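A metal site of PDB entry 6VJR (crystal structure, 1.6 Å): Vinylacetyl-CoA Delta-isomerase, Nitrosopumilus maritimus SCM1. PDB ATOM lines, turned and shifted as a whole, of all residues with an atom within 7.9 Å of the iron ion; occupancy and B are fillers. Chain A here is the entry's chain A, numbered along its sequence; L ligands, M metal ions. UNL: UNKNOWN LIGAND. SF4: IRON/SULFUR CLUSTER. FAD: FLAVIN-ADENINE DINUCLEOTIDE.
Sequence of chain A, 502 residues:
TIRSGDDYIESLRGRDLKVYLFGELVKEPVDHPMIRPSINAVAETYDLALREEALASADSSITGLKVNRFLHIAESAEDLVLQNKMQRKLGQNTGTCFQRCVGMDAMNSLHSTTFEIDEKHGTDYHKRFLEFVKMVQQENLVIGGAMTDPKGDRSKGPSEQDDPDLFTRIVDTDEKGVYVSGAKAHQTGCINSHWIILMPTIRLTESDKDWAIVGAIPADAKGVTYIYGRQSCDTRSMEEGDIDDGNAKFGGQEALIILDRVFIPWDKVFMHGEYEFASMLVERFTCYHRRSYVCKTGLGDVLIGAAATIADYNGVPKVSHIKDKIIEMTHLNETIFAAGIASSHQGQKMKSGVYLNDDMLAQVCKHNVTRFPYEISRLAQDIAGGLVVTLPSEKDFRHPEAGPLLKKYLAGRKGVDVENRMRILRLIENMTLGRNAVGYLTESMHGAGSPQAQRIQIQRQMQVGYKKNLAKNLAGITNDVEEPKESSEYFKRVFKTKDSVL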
ATOM      1  N   CYS A  97       3.979   0.631 -30.348  1.00  0.00           N
ATOM      2  CA  CYS A  97       3.947  -0.678 -30.949  1.00  0.00           C
ATOM      3  C   CYS A  97       4.899  -0.745 -32.153  1.00  0.00           C
ATOM      4  O   CYS A  97       4.664  -0.067 -33.141  1.00  0.00           O
ATOM      5  CB  CYS A  97       2.524  -1.032 -31.368  1.00  0.00           C
ATOM      6  SG  CYS A  97       2.487  -2.596 -32.301  1.00  0.00           S
ATOM      7  N   CYS A 101       6.245  -8.325 -33.623  1.00  0.00           N
ATOM      8  CA  CYS A 101       6.013  -9.435 -32.696  1.00  0.00           C
ATOM      9  C   CYS A 101       4.952 -10.367 -33.297  1.00  0.00           C
ATOM     10  O   CYS A 101       5.003 -11.568 -33.093  1.00  0.00           O
ATOM     11  CB  CYS A 101       5.535  -8.992 -31.310  1.00  0.00           C
ATOM     12  SG  CYS A 101       6.603  -7.714 -30.610  1.00  0.00           S
ATOM     13  N   VAL A 102       3.904  -9.812 -33.953  1.00  0.00           N
ATOM     14  CA  VAL A 102       2.788 -10.645 -34.412  1.00  0.00           C
ATOM     15  C   VAL A 102       3.273 -11.744 -35.364  1.00  0.00           C
ATOM     16  O   VAL A 102       2.932 -12.936 -35.245  1.00  0.00           O
ATOM     17  CB  VAL A 102       1.690  -9.793 -35.065  1.00  0.00           C
ATOM     18  CG1 VAL A 102       0.420 -10.600 -35.175  1.00  0.00           C
ATOM     19  CG2 VAL A 102       1.421  -8.527 -34.306  1.00  0.00           C
ATOM     20  N   ASP A 105       5.321 -14.485 -33.574  1.00  0.00           N
ATOM     21  CA  ASP A 105       4.449 -15.426 -32.864  1.00  0.00           C
ATOM     22  C   ASP A 105       3.691 -16.318 -33.852  1.00  0.00           C
ATOM     23  O   ASP A 105       3.486 -17.516 -33.599  1.00  0.00           O
ATOM     24  CB  ASP A 105       3.614 -14.608 -31.905  1.00  0.00           C
ATOM     25  CG  ASP A 105       4.412 -13.932 -30.770  1.00  0.00           C
ATOM     26  OD1 ASP A 105       5.494 -14.467 -30.379  1.00  0.00           O
ATOM     27  OD2 ASP A 105       3.918 -12.918 -30.208  1.00  0.00           O
ATOM     28  N   THR A 188      -1.843  -4.994 -37.528  1.00  0.00           N
ATOM     29  CA  THR A 188      -0.697  -4.239 -37.069  1.00  0.00           C
ATOM     30  C   THR A 188       0.400  -4.271 -38.121  1.00  0.00           C
ATOM     31  O   THR A 188       0.893  -5.333 -38.468  1.00  0.00           O
ATOM     32  CB  THR A 188      -0.226  -4.809 -35.706  1.00  0.00           C
ATOM     33  OG1 THR A 188      -1.246  -4.585 -34.728  1.00  0.00           O
ATOM     34  CG2 THR A 188       1.047  -4.155 -35.233  1.00  0.00           C
ATOM     35  N   PHE A 285      -0.752 -19.640 -31.262  1.00  0.00           N
ATOM     36  CA  PHE A 285      -0.463 -18.249 -31.578  1.00  0.00           C
ATOM     37  C   PHE A 285      -0.737 -17.367 -30.381  1.00  0.00           C
ATOM     38  O   PHE A 285       0.116 -16.540 -29.967  1.00  0.00           O
ATOM     39  CB  PHE A 285      -1.252 -17.764 -32.789  1.00  0.00           C
ATOM     40  CG  PHE A 285      -1.153 -16.273 -32.950  1.00  0.00           C
ATOM     41  CD1 PHE A 285       0.024 -15.685 -33.375  1.00  0.00           C
ATOM     42  CD2 PHE A 285      -2.171 -15.460 -32.456  1.00  0.00           C
ATOM     43  CE1 PHE A 285       0.117 -14.330 -33.512  1.00  0.00           C
ATOM     44  CE2 PHE A 285      -2.067 -14.082 -32.552  1.00  0.00           C
ATOM     45  CZ  PHE A 285      -0.924 -13.507 -33.047  1.00  0.00           C
ATOM     46  N   HIS A 289       1.612 -14.998 -28.110  1.00  0.00           N
ATOM     47  CA  HIS A 289       1.369 -13.568 -28.211  1.00  0.00           C
ATOM     48  C   HIS A 289       0.914 -12.964 -26.868  1.00  0.00           C
ATOM     49  O   HIS A 289       1.274 -11.820 -26.573  1.00  0.00           O
ATOM     50  CB  HIS A 289       0.433 -13.220 -29.349  1.00  0.00           C
ATOM     51  CG  HIS A 289       0.591 -11.800 -29.770  1.00  0.00           C
ATOM     52  ND1 HIS A 289       1.758 -11.251 -30.262  1.00  0.00           N
ATOM     53  CD2 HIS A 289      -0.288 -10.775 -29.682  1.00  0.00           C
ATOM     54  CE1 HIS A 289       1.543  -9.931 -30.449  1.00  0.00           C
ATOM     55  NE2 HIS A 289       0.301  -9.623 -30.105  1.00  0.00           N
ATOM     56  N   ARG A 290       0.192 -13.733 -26.055  1.00  0.00           N
ATOM     57  CA  ARG A 290      -0.310 -13.260 -24.770  1.00  0.00           C
ATOM     58  C   ARG A 290       0.845 -12.941 -23.812  1.00  0.00           C
ATOM     59  O   ARG A 290       0.689 -12.150 -22.908  1.00  0.00           O
ATOM     60  CB  ARG A 290      -1.319 -14.241 -24.192  1.00  0.00           C
ATOM     61  CG  ARG A 290      -2.664 -14.058 -24.878  1.00  0.00           C
ATOM     62  CD  ARG A 290      -3.741 -15.001 -24.467  1.00  0.00           C
ATOM     63  NE  ARG A 290      -4.948 -14.773 -25.257  1.00  0.00           N
ATOM     64  CZ  ARG A 290      -5.886 -15.676 -25.457  1.00  0.00           C
ATOM     65  NH1 ARG A 290      -5.929 -16.757 -24.713  1.00  0.00           N
ATOM     66  NH2 ARG A 290      -6.751 -15.507 -26.410  1.00  0.00           N
ATOM     67  N   SER A 292       3.964 -11.892 -25.292  1.00  0.00           N
ATOM     68  CA  SER A 292       4.664 -10.833 -25.997  1.00  0.00           C
ATOM     69  C   SER A 292       4.340  -9.461 -25.431  1.00  0.00           C
ATOM     70  O   SER A 292       5.094  -8.500 -25.674  1.00  0.00           O
ATOM     71  CB  SER A 292       4.448 -10.948 -27.500  1.00  0.00           C
ATOM     72  OG  SER A 292       5.191 -12.080 -27.973  1.00  0.00           O
ATOM     73  N   TYR A 293       3.255  -9.401 -24.647  1.00  0.00           N
ATOM     74  CA  TYR A 293       2.839  -8.155 -23.967  1.00  0.00           C
ATOM     75  C   TYR A 293       3.832  -7.679 -22.912  1.00  0.00           C
ATOM     76  O   TYR A 293       3.631  -6.613 -22.349  1.00  0.00           O
ATOM     77  CB  TYR A 293       1.405  -8.204 -23.411  1.00  0.00           C
ATOM     78  CG  TYR A 293       0.454  -8.205 -24.586  1.00  0.00           C
ATOM     79  CD1 TYR A 293       0.012  -7.010 -25.138  1.00  0.00           C
ATOM     80  CD2 TYR A 293       0.043  -9.391 -25.161  1.00  0.00           C
ATOM     81  CE1 TYR A 293      -0.749  -6.983 -26.284  1.00  0.00           C
ATOM     82  CE2 TYR A 293      -0.723  -9.388 -26.312  1.00  0.00           C
ATOM     83  CZ  TYR A 293      -1.066  -8.180 -26.887  1.00  0.00           C
ATOM     84  OH  TYR A 293      -1.711  -8.173 -28.059  1.00  0.00           O
ATOM     85  N   CYS A 295       6.210  -6.343 -24.034  1.00  0.00           N
ATOM     86  CA  CYS A 295       6.504  -5.100 -24.740  1.00  0.00           C
ATOM     87  C   CYS A 295       5.901  -3.897 -24.000  1.00  0.00           C
ATOM     88  O   CYS A 295       6.507  -2.839 -23.891  1.00  0.00           O
ATOM     89  CB  CYS A 295       6.044  -5.142 -26.203  1.00  0.00           C
ATOM     90  SG  CYS A 295       4.247  -5.235 -26.392  1.00  0.00           S
ATOM     91  N   LYS A 296       4.725  -4.079 -23.392  1.00  0.00           N
ATOM     92  CA  LYS A 296       4.022  -2.995 -22.746  1.00  0.00           C
ATOM     93  C   LYS A 296       4.720  -2.558 -21.456  1.00  0.00           C
ATOM     94  O   LYS A 296       4.479  -1.459 -20.953  1.00  0.00           O
ATOM     95  CB  LYS A 296       2.606  -3.431 -22.360  1.00  0.00           C
ATOM     96  CG  LYS A 296       1.735  -3.853 -23.535  1.00  0.00           C
ATOM     97  CD  LYS A 296       1.518  -2.849 -24.641  1.00  0.00           C
ATOM     98  CE  LYS A 296       0.762  -3.520 -25.776  1.00  0.00           C
ATOM     99  NZ  LYS A 296       0.587  -2.631 -26.911  1.00  0.00           N
ATOM    100  N   LYS A 366      -1.214 -11.682 -19.954  1.00  0.00           N
ATOM    101  CA  LYS A 366      -2.142 -10.874 -20.744  1.00  0.00           C
ATOM    102  C   LYS A 366      -3.301 -10.382 -19.891  1.00  0.00           C
ATOM    103  O   LYS A 366      -3.751  -9.249 -20.060  1.00  0.00           O
ATOM    104  CB  LYS A 366      -2.620 -11.725 -21.927  1.00  0.00           C
ATOM    105  CG  LYS A 366      -3.935 -11.258 -22.476  1.00  0.00           C
ATOM    106  CD  LYS A 366      -3.846  -9.966 -23.278  1.00  0.00           C
ATOM    107  CE  LYS A 366      -5.191  -9.729 -23.835  1.00  0.00           C
ATOM    108  NZ  LYS A 366      -5.368  -8.479 -24.532  1.00  0.00           N
ATOM    109  N   GLY A 439      -2.317   1.766 -28.590  1.00  0.00           N
ATOM    110  CA  GLY A 439      -1.561   0.571 -28.292  1.00  0.00           C
ATOM    111  C   GLY A 439      -1.427   0.304 -26.795  1.00  0.00           C
ATOM    112  O   GLY A 439      -1.663  -0.823 -26.347  1.00  0.00           O
ATOM    113  N   GLU A 443      -5.009  -1.812 -27.217  1.00  0.00           N
ATOM    114  CA  GLU A 443      -4.431  -3.050 -27.705  1.00  0.00           C
ATOM    115  C   GLU A 443      -4.035  -3.948 -26.534  1.00  0.00           C
ATOM    116  O   GLU A 443      -4.138  -5.156 -26.624  1.00  0.00           O
ATOM    117  CB  GLU A 443      -3.235  -2.785 -28.603  1.00  0.00           C
ATOM    118  CG  GLU A 443      -3.001  -3.997 -29.507  1.00  0.00           C
ATOM    119  CD  GLU A 443      -1.974  -4.966 -29.062  1.00  0.00           C
ATOM    120  OE1 GLU A 443      -1.145  -4.538 -28.206  1.00  0.00           O
ATOM    121  OE2 GLU A 443      -1.958  -6.084 -29.623  1.00  0.00           O
ATOM    122  N   SER A 444      -3.652  -3.369 -25.385  1.00  0.00           N
ATOM    123  CA  SER A 444      -3.481  -4.168 -24.169  1.00  0.00           C
ATOM    124  C   SER A 444      -4.767  -4.918 -23.832  1.00  0.00           C
ATOM    125  O   SER A 444      -4.779  -6.064 -23.405  1.00  0.00           O
ATOM    126  CB  SER A 444      -2.975  -3.318 -23.002  1.00  0.00           C
ATOM    127  OG  SER A 444      -1.644  -2.892 -23.250  1.00  0.00           O
ATOM    128  N   HIS A 446      -7.341  -5.775 -26.030  1.00  0.00           N
ATOM    129  CA  HIS A 446      -7.897  -6.694 -27.044  1.00  0.00           C
ATOM    130  C   HIS A 446      -6.880  -7.550 -27.796  1.00  0.00           C
ATOM    131  O   HIS A 446      -7.236  -8.535 -28.425  1.00  0.00           O
ATOM    132  CB  HIS A 446      -8.746  -5.943 -28.073  1.00  0.00           C
ATOM    133  CG  HIS A 446     -10.037  -5.470 -27.461  1.00  0.00           C
ATOM    134  ND1 HIS A 446     -10.949  -6.367 -26.966  1.00  0.00           N
ATOM    135  CD2 HIS A 446     -10.497  -4.262 -27.170  1.00  0.00           C
ATOM    136  CE1 HIS A 446     -11.985  -5.708 -26.450  1.00  0.00           C
ATOM    137  NE2 HIS A 446     -11.743  -4.400 -26.573  1.00  0.00           N
ATOM    138  N   GLY A 447      -5.646  -7.151 -27.791  1.00  0.00           N
ATOM    139  CA  GLY A 447      -4.629  -7.885 -28.539  1.00  0.00           C
ATOM    140  C   GLY A 447      -4.489  -9.351 -28.091  1.00  0.00           C
ATOM    141  O   GLY A 447      -4.477  -9.662 -26.906  1.00  0.00           O
ATOM    142  N   ALA A 448      -4.474 -10.273 -29.057  1.00  0.00           N
ATOM    143  CA  ALA A 448      -4.542 -11.727 -28.833  1.00  0.00           C
ATOM    144  C   ALA A 448      -5.782 -12.157 -28.043  1.00  0.00           C
ATOM    145  O   ALA A 448      -5.806 -13.214 -27.384  1.00  0.00           O
ATOM    146  CB  ALA A 448      -3.321 -12.241 -28.123  1.00  0.00           C
ATOM    147  N   GLY A 449      -6.831 -11.371 -28.159  1.00  0.00           N
ATOM    148  CA  GLY A 449      -8.116 -11.716 -27.590  1.00  0.00           C
ATOM    149  C   GLY A 449      -8.498 -10.817 -26.421  1.00  0.00           C
ATOM    150  O   GLY A 449      -7.689 -10.402 -25.585  1.00  0.00           O
HETATM  151  O2  UNL L   1      -4.284  -9.890 -31.829  1.00  0.00           O
HETATM  152  C1  UNL L   1      -2.798  -9.510 -32.074  1.00  0.00           C
HETATM  153  O1  UNL L   1      -2.261  -8.494 -31.061  1.00  0.00           O
HETATM  154 FE1  SF4 L   2       1.916  -6.484 -29.917  1.00  0.00          FE
HETATM  155 FE2  SF4 L   2       3.441  -4.823 -28.349  1.00  0.00          FE
HETATM  156 FE3  SF4 L   2       3.102  -4.245 -30.864  1.00  0.00          FE
HETATM  157 FE4  SF4 L   2       4.777  -6.228 -30.189  1.00  0.00          FE
HETATM  158  S1  SF4 L   2       5.082  -4.040 -29.813  1.00  0.00           S
HETATM  159  S2  SF4 L   2       3.139  -6.298 -31.872  1.00  0.00           S
HETATM  160  S3  SF4 L   2       3.578  -7.138 -28.395  1.00  0.00           S
HETATM  161  S4  SF4 L   2       1.414  -4.402 -29.336  1.00  0.00           S
HETATM  162  PA  FAD L   3     -15.206  -8.486 -30.263  1.00  0.00           P
HETATM  163  O1A FAD L   3     -15.004  -9.920 -30.464  1.00  0.00           O
HETATM  164  O2A FAD L   3     -16.287  -7.826 -31.025  1.00  0.00           O
HETATM  165  O5B FAD L   3     -15.252  -8.260 -28.678  1.00  0.00           O
HETATM  166  C5B FAD L   3     -16.128  -7.277 -28.068  1.00  0.00           C
HETATM  167  C4B FAD L   3     -16.647  -7.848 -26.781  1.00  0.00           C
HETATM  168  O4B FAD L   3     -17.601  -8.906 -27.073  1.00  0.00           O
HETATM  169  C3B FAD L   3     -15.616  -8.452 -25.820  1.00  0.00           C
HETATM  170  O3B FAD L   3     -15.981  -8.180 -24.462  1.00  0.00           O
HETATM  171  C2B FAD L   3     -15.719  -9.949 -26.105  1.00  0.00           C
HETATM  172  O2B FAD L   3     -15.296 -10.827 -25.072  1.00  0.00           O
HETATM  173  C1B FAD L   3     -17.219 -10.085 -26.390  1.00  0.00           C
HETATM  174  N9A FAD L   3     -17.558 -11.204 -27.261  1.00  0.00           N
HETATM  175  C8A FAD L   3     -17.274 -11.400 -28.592  1.00  0.00           C
HETATM  176  N7A FAD L   3     -17.744 -12.508 -29.103  1.00  0.00           N
HETATM  177  C5A FAD L   3     -18.351 -13.116 -28.025  1.00  0.00           C
HETATM  178  C6A FAD L   3     -19.044 -14.339 -27.899  1.00  0.00           C
HETATM  179  N6A FAD L   3     -19.272 -15.143 -28.941  1.00  0.00           N
HETATM  180  N1A FAD L   3     -19.490 -14.695 -26.669  1.00  0.00           N
HETATM  181  C2A FAD L   3     -19.283 -13.841 -25.649  1.00  0.00           C
HETATM  182  N3A FAD L   3     -18.678 -12.651 -25.642  1.00  0.00           N
HETATM  183  C4A FAD L   3     -18.221 -12.335 -26.877  1.00  0.00           C
HETATM  184  N1  FAD L   3      -5.435  -9.125 -34.847  1.00  0.00           N
HETATM  185  C2  FAD L   3      -4.657  -9.704 -35.821  1.00  0.00           C
HETATM  186  O2  FAD L   3      -4.976 -10.763 -36.395  1.00  0.00           O
HETATM  187  N3  FAD L   3      -3.445  -9.116 -36.136  1.00  0.00           N
HETATM  188  C4  FAD L   3      -2.928  -7.979 -35.596  1.00  0.00           C
HETATM  189  O4  FAD L   3      -1.898  -7.473 -36.007  1.00  0.00           O
HETATM  190  C4X FAD L   3      -3.814  -7.331 -34.635  1.00  0.00           C
HETATM  191  N5  FAD L   3      -3.412  -6.192 -34.070  1.00  0.00           N
HETATM  192  C5X FAD L   3      -4.334  -5.475 -33.343  1.00  0.00           C
HETATM  193  C6  FAD L   3      -4.059  -4.166 -32.915  1.00  0.00           C
HETATM  194  C7  FAD L   3      -4.992  -3.414 -32.224  1.00  0.00           C
HETATM  195  C7M FAD L   3      -4.683  -1.970 -31.884  1.00  0.00           C
HETATM  196  C8  FAD L   3      -6.190  -4.011 -31.803  1.00  0.00           C
HETATM  197  C8M FAD L   3      -7.168  -3.241 -30.956  1.00  0.00           C
HETATM  198  C9  FAD L   3      -6.458  -5.317 -32.129  1.00  0.00           C
HETATM  199  C9A FAD L   3      -5.555  -6.057 -32.934  1.00  0.00           C
HETATM  200  N10 FAD L   3      -5.847  -7.338 -33.378  1.00  0.00           N
HETATM  201  C10 FAD L   3      -5.046  -7.992 -34.323  1.00  0.00           C
HETATM  202  C1' FAD L   3      -7.238  -7.805 -33.169  1.00  0.00           C
HETATM  203  C2' FAD L   3      -7.591  -8.393 -31.822  1.00  0.00           C
HETATM  204  O2' FAD L   3      -7.123  -9.739 -31.803  1.00  0.00           O
HETATM  205  C3' FAD L   3      -9.107  -8.350 -31.630  1.00  0.00           C
HETATM  206  O3' FAD L   3      -9.450  -6.984 -31.444  1.00  0.00           O
HETATM  207  C4' FAD L   3      -9.650  -9.255 -30.507  1.00  0.00           C
HETATM  208  O4' FAD L   3      -9.538 -10.642 -30.878  1.00  0.00           O
HETATM  209  C5' FAD L   3     -11.096  -8.965 -30.160  1.00  0.00           C
HETATM  210  O5' FAD L   3     -11.901  -9.107 -31.316  1.00  0.00           O
HETATM  211  P   FAD L   3     -12.842  -7.963 -31.799  1.00  0.00           P
HETATM  212  O1P FAD L   3     -12.111  -6.697 -31.998  1.00  0.00           O
HETATM  213  O2P FAD L   3     -13.628  -8.504 -32.921  1.00  0.00           O
HETATM  214  O3P FAD L   3     -13.859  -7.653 -30.605  1.00  0.00           O
HETATM  215 FE    FE M   1      -0.860  -7.685 -29.803  1.00  0.00          FE
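Gly 447 touches the iron ion.
Within 4 Å of the iron ion: His 289, Tyr 293, Glu 443 and Gly 447.
The nearest printed residue that does not touch the iron ion is Ala 448 (4.5 Å).
OE2 of Glu 443 binds the iron ion (1.9 Å).
OH of Tyr 293 is bound to the iron ion (2.0 Å).
The iron ion is bound by O1 of UNL L1 (2.0 Å).
A ring nitrogen (NE2) of His 289 is bound to the iron ion (2.3 Å).
The side-chain amino group (NZ) of Lys 366 sits at hydrogen-bond distance from the backbone carbonyl oxygen (O) of Gly 447 (2.8 Å).
The side-chain hydroxyl (OH) of Tyr 293 sits close to the backbone carbonyl oxygen (O) of Gly 447, at 3.3 Å.
The side-chain amino group of Lys 296 is in salt-bridge range of the side-chain carboxylate of Glu 443 (2.9 Å).
A ring nitrogen (ND1) of His 289 sits at hydrogen-bond distance from the side-chain carboxylate of Asp 105 (2.7 Å).
The backbone NH (N) of Thr 188 lies within hydrogen-bond range of an oxygen (O4) of FAD L3.
FE3 of SF4 L2 is bound by SG of Cys 97 (2.3 Å).
The side-chain hydroxyl of Thr 188 is in hydrogen-bond range of a nitrogen (N5) of FAD L3 (2.8 Å).
The side-chain sulfur of Cys 295 binds an iron atom (FE2) of SF4 L2 (2.2 Å).
S4 of SF4 L2 lies close to NZ of Lys 296 (3.1 Å).
The side-chain sulfur of Cys 101 is bound to an iron atom (FE4) of SF4 L2, 2.4 Å away.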
